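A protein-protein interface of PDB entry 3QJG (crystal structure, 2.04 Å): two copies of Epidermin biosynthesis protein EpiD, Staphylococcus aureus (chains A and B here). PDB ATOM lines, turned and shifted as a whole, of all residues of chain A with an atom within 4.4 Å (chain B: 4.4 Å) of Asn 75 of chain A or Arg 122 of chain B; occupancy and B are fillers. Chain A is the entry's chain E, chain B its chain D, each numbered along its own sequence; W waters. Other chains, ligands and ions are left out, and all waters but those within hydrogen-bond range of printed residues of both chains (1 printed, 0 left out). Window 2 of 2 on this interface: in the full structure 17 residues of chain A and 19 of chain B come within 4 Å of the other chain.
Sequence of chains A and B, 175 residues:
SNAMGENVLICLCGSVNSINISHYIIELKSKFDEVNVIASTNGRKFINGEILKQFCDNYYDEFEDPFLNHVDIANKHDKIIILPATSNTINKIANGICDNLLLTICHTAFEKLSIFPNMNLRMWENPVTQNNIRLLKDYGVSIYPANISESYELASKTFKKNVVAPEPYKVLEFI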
ATOM      1  N   VAL A  71     -20.522  13.758  30.164  1.00  0.00           N
ATOM      2  CA  VAL A  71     -19.829  14.935  30.728  1.00  0.00           C
ATOM      3  C   VAL A  71     -20.122  14.936  32.222  1.00  0.00           C
ATOM      4  O   VAL A  71     -19.205  15.051  33.065  1.00  0.00           O
ATOM      5  CB  VAL A  71     -20.267  16.258  30.043  1.00  0.00           C
ATOM      6  CG1 VAL A  71     -19.711  17.456  30.761  1.00  0.00           C
ATOM      7  CG2 VAL A  71     -19.837  16.271  28.587  1.00  0.00           C
ATOM      8  N   ASP A  72     -21.385  14.741  32.554  1.00  0.00           N
ATOM      9  CA  ASP A  72     -21.733  14.754  33.986  1.00  0.00           C
ATOM     10  C   ASP A  72     -21.093  13.600  34.741  1.00  0.00           C
ATOM     11  O   ASP A  72     -20.611  13.791  35.851  1.00  0.00           O
ATOM     12  CB  ASP A  72     -23.234  14.806  34.217  1.00  0.00           C
ATOM     13  CG  ASP A  72     -23.883  16.008  33.508  1.00  0.00           C
ATOM     14  OD1 ASP A  72     -23.214  17.087  33.361  1.00  0.00           O
ATOM     15  OD2 ASP A  72     -25.051  15.862  33.091  1.00  0.00           O
ATOM     16  N   ILE A  73     -21.063  12.413  34.150  1.00  0.00           N
ATOM     17  CA  ILE A  73     -20.436  11.279  34.816  1.00  0.00           C
ATOM     18  C   ILE A  73     -18.921  11.540  35.008  1.00  0.00           C
ATOM     19  O   ILE A  73     -18.416  11.296  36.078  1.00  0.00           O
ATOM     20  CB  ILE A  73     -20.649   9.988  34.036  1.00  0.00           C
ATOM     21  CG1 ILE A  73     -22.132   9.565  34.092  1.00  0.00           C
ATOM     22  CG2 ILE A  73     -19.681   8.894  34.523  1.00  0.00           C
ATOM     23  CD1 ILE A  73     -22.458   8.451  33.202  1.00  0.00           C
ATOM     24  N   ALA A  74     -18.229  12.038  33.985  1.00  0.00           N
ATOM     25  CA  ALA A  74     -16.754  12.329  34.080  1.00  0.00           C
ATOM     26  C   ALA A  74     -16.458  13.374  35.111  1.00  0.00           C
ATOM     27  O   ALA A  74     -15.440  13.270  35.891  1.00  0.00           O
ATOM     28  CB  ALA A  74     -16.201  12.798  32.736  1.00  0.00           C
ATOM     29  N   ASN A  75     -17.270  14.434  35.085  1.00  0.00           N
ATOM     30  CA  ASN A  75     -17.142  15.535  36.062  1.00  0.00           C
ATOM     31  C   ASN A  75     -17.320  15.124  37.511  1.00  0.00           C
ATOM     32  O   ASN A  75     -16.813  15.790  38.396  1.00  0.00           O
ATOM     33  CB  ASN A  75     -18.128  16.668  35.731  1.00  0.00           C
ATOM     34  CG  ASN A  75     -17.678  17.496  34.531  1.00  0.00           C
ATOM     35  OD1 ASN A  75     -16.511  17.427  34.097  1.00  0.00           O
ATOM     36  ND2 ASN A  75     -18.605  18.272  33.981  1.00  0.00           N
ATOM     37  N   LYS A  76     -18.063  14.053  37.764  1.00  0.00           N
ATOM     38  CA  LYS A  76     -18.246  13.552  39.139  1.00  0.00           C
ATOM     39  C   LYS A  76     -16.983  12.849  39.732  1.00  0.00           C
ATOM     40  O   LYS A  76     -16.914  12.577  40.945  1.00  0.00           O
ATOM     41  CB  LYS A  76     -19.397  12.569  39.147  1.00  0.00           C
ATOM     42  CG  LYS A  76     -19.902  12.193  40.517  1.00  0.00           C
ATOM     43  CD  LYS A  76     -20.935  11.052  40.428  1.00  0.00           C
ATOM     44  CE  LYS A  76     -21.825  11.037  41.663  1.00  0.00           C
ATOM     45  NZ  LYS A  76     -22.193   9.666  42.116  1.00  0.00           N
ATOM     46  N   HIS A  77     -15.992  12.546  38.897  1.00  0.00           N
ATOM     47  CA  HIS A  77     -14.897  11.665  39.307  1.00  0.00           C
ATOM     48  C   HIS A  77     -13.537  12.320  39.230  1.00  0.00           C
ATOM     49  O   HIS A  77     -13.186  12.982  38.251  1.00  0.00           O
ATOM     50  CB  HIS A  77     -14.922  10.397  38.451  1.00  0.00           C
ATOM     51  CG  HIS A  77     -16.160   9.585  38.640  1.00  0.00           C
ATOM     52  ND1 HIS A  77     -17.310   9.804  37.923  1.00  0.00           N
ATOM     53  CD2 HIS A  77     -16.456   8.615  39.534  1.00  0.00           C
ATOM     54  CE1 HIS A  77     -18.246   8.969  38.328  1.00  0.00           C
ATOM     55  NE2 HIS A  77     -17.755   8.233  39.304  1.00  0.00           N
ATOM     56  N   THR A 108     -13.794  12.251  27.056  1.00  0.00           N
ATOM     57  CA  THR A 108     -13.977  13.551  27.697  1.00  0.00           C
ATOM     58  C   THR A 108     -12.973  13.864  28.833  1.00  0.00           C
ATOM     59  O   THR A 108     -12.941  14.986  29.332  1.00  0.00           O
ATOM     60  CB  THR A 108     -15.402  13.628  28.190  1.00  0.00           C
ATOM     61  OG1 THR A 108     -16.295  13.520  27.048  1.00  0.00           O
ATOM     62  CG2 THR A 108     -15.669  14.900  28.947  1.00  0.00           C
ATOM     63  N   LYS A 112      -7.740  12.675  33.516  1.00  0.00           N
ATOM     64  CA  LYS A 112      -8.123  11.906  34.707  1.00  0.00           C
ATOM     65  C   LYS A 112      -7.930  10.390  34.497  1.00  0.00           C
ATOM     66  O   LYS A 112      -8.230   9.610  35.385  1.00  0.00           O
ATOM     67  CB  LYS A 112      -9.600  12.150  35.067  1.00  0.00           C
ATOM     68  CG  LYS A 112     -10.070  13.576  35.434  1.00  0.00           C
ATOM     69  CD  LYS A 112     -11.621  13.513  35.546  1.00  0.00           C
ATOM     70  CE  LYS A 112     -12.316  14.837  35.659  1.00  0.00           C
ATOM     71  NZ  LYS A 112     -12.946  15.020  36.964  1.00  0.00           N
ATOM     72  N   ASN B 120     -19.346  18.935  23.689  1.00  0.00           N
ATOM     73  CA  ASN B 120     -18.617  19.545  24.781  1.00  0.00           C
ATOM     74  C   ASN B 120     -17.187  20.017  24.444  1.00  0.00           C
ATOM     75  O   ASN B 120     -16.440  19.338  23.746  1.00  0.00           O
ATOM     76  CB  ASN B 120     -18.501  18.587  25.947  1.00  0.00           C
ATOM     77  CG  ASN B 120     -18.109  19.286  27.184  1.00  0.00           C
ATOM     78  OD1 ASN B 120     -16.974  19.212  27.617  1.00  0.00           O
ATOM     79  ND2 ASN B 120     -19.035  20.005  27.751  1.00  0.00           N
ATOM     80  N   LEU B 121     -16.802  21.165  25.003  1.00  0.00           N
ATOM     81  CA  LEU B 121     -15.450  21.696  24.770  1.00  0.00           C
ATOM     82  C   LEU B 121     -14.325  20.692  25.096  1.00  0.00           C
ATOM     83  O   LEU B 121     -13.325  20.645  24.407  1.00  0.00           O
ATOM     84  CB  LEU B 121     -15.227  23.020  25.508  1.00  0.00           C
ATOM     85  CG  LEU B 121     -13.976  23.803  25.097  1.00  0.00           C
ATOM     86  CD1 LEU B 121     -13.868  23.931  23.587  1.00  0.00           C
ATOM     87  CD2 LEU B 121     -13.972  25.179  25.727  1.00  0.00           C
ATOM     88  N   ARG B 122     -14.489  19.863  26.107  1.00  0.00           N
ATOM     89  CA  ARG B 122     -13.435  18.903  26.400  1.00  0.00           C
ATOM     90  C   ARG B 122     -13.322  17.879  25.258  1.00  0.00           C
ATOM     91  O   ARG B 122     -12.250  17.398  24.977  1.00  0.00           O
ATOM     92  CB  ARG B 122     -13.630  18.234  27.765  1.00  0.00           C
ATOM     93  CG  ARG B 122     -13.296  19.146  28.935  1.00  0.00           C
ATOM     94  CD  ARG B 122     -13.117  18.358  30.225  1.00  0.00           C
ATOM     95  NE  ARG B 122     -13.518  19.108  31.421  1.00  0.00           N
ATOM     96  CZ  ARG B 122     -14.779  19.404  31.762  1.00  0.00           C
ATOM     97  NH1 ARG B 122     -15.813  19.030  31.008  1.00  0.00           N
ATOM     98  NH2 ARG B 122     -15.009  20.103  32.867  1.00  0.00           N
ATOM     99  N   MET B 123     -14.415  17.598  24.557  1.00  0.00           N
ATOM    100  CA  MET B 123     -14.354  16.614  23.502  1.00  0.00           C
ATOM    101  C   MET B 123     -13.758  17.315  22.252  1.00  0.00           C
ATOM    102  O   MET B 123     -12.920  16.747  21.557  1.00  0.00           O
ATOM    103  CB  MET B 123     -15.715  15.978  23.296  1.00  0.00           C
ATOM    104  CG  MET B 123     -16.377  15.337  24.576  1.00  0.00           C
ATOM    105  SD  MET B 123     -18.134  15.204  24.171  1.00  0.00           S
ATOM    106  CE  MET B 123     -18.124  13.771  23.112  1.00  0.00           C
ATOM    107  N   TRP B 124     -14.092  18.583  22.039  1.00  0.00           N
ATOM    108  CA  TRP B 124     -13.477  19.380  20.956  1.00  0.00           C
ATOM    109  C   TRP B 124     -11.968  19.616  21.134  1.00  0.00           C
ATOM    110  O   TRP B 124     -11.188  19.499  20.185  1.00  0.00           O
ATOM    111  CB  TRP B 124     -14.172  20.721  20.858  1.00  0.00           C
ATOM    112  CG  TRP B 124     -13.757  21.573  19.719  1.00  0.00           C
ATOM    113  CD1 TRP B 124     -13.181  22.796  19.804  1.00  0.00           C
ATOM    114  CD2 TRP B 124     -13.947  21.312  18.321  1.00  0.00           C
ATOM    115  NE1 TRP B 124     -12.978  23.314  18.553  1.00  0.00           N
ATOM    116  CE2 TRP B 124     -13.430  22.423  17.619  1.00  0.00           C
ATOM    117  CE3 TRP B 124     -14.498  20.244  17.591  1.00  0.00           C
ATOM    118  CZ2 TRP B 124     -13.431  22.498  16.219  1.00  0.00           C
ATOM    119  CZ3 TRP B 124     -14.506  20.314  16.199  1.00  0.00           C
ATOM    120  CH2 TRP B 124     -13.973  21.436  15.526  1.00  0.00           C
ATOM    121  N   GLU B 125     -11.559  19.949  22.336  1.00  0.00           N
ATOM    122  CA  GLU B 125     -10.122  20.159  22.617  1.00  0.00           C
ATOM    123  C   GLU B 125      -9.342  18.898  22.920  1.00  0.00           C
ATOM    124  O   GLU B 125      -8.161  18.963  23.267  1.00  0.00           O
ATOM    125  CB  GLU B 125      -9.964  21.172  23.755  1.00  0.00           C
ATOM    126  CG  GLU B 125     -10.403  22.565  23.311  1.00  0.00           C
ATOM    127  CD  GLU B 125     -10.478  23.564  24.437  1.00  0.00           C
ATOM    128  OE1 GLU B 125     -10.445  23.146  25.623  1.00  0.00           O
ATOM    129  OE2 GLU B 125     -10.578  24.773  24.114  1.00  0.00           O
ATOM    130  N   ASN B 126      -9.999  17.735  22.842  1.00  0.00           N
ATOM    131  CA  ASN B 126      -9.263  16.462  22.916  1.00  0.00           C
ATOM    132  C   ASN B 126      -8.330  16.457  21.703  1.00  0.00           C
ATOM    133  O   ASN B 126      -8.767  16.764  20.587  1.00  0.00           O
ATOM    134  CB  ASN B 126     -10.211  15.261  22.949  1.00  0.00           C
ATOM    135  CG  ASN B 126      -9.462  13.942  23.001  1.00  0.00           C
ATOM    136  OD1 ASN B 126      -8.516  13.721  22.214  1.00  0.00           O
ATOM    137  ND2 ASN B 126      -9.886  13.042  23.911  1.00  0.00           N
HETATM  138  O   HOH W   1     -12.315  16.166  31.877  1.00  0.00           O
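Of the printed residues of chain B, Asn 75 of chain A touches Arg 122.
Of the printed residues of chain A, Arg 122 of chain B touches Asn 75 and Thr 108.
Printed residues of chain B within 4 Å of Thr 108 of chain A: Arg 122 and Met 123.
Printed residues of chain A within 4 Å of Asn 120 of chain B: Val 71 (3.7 Å).
Asp 72 of chain A touches none of the printed residues of chain B.
Leu 121 of chain B touches none of the printed residues of chain A.
The nearest printed residue of chain B that does not touch Asn 75 of chain A is Asn 120 of chain B (6.5 Å).
The nearest printed residue of chain B that does not touch Val 71 of chain A is Arg 122 of chain B (4.2 Å).
Water W1 lies within hydrogen-bond range of O of Thr 108 of chain A and NE of Arg 122 of chain B.
The side-chain amide oxygen of Asn 120 of chain B lies within hydrogen-bond range of the backbone NH of Arg 122 of chain B, 3.0 Å away.
O of Val 71 of chain A lies close to ND2 of Asn 75 of chain A (3.4 Å).
The side-chain amide oxygen (OD1) of Asn 75 of chain A lies within hydrogen-bond range of the guanidinium group (NH2) of Arg 122 of chain B (3.3 Å).
No position is printed for both chains.
Of the 4 pairs that touch across the chains among the printed residues, none has its exchanged pair printed and touching as well.
CG2 of Val 71 of chain A touches CG of Asn 120 of chain B, 3.7 Å away.
O of Thr 108 of chain A touches CD of Arg 122 of chain B, at 3.5 Å.
Thr 108 of chain A touches Met 123 of chain B.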
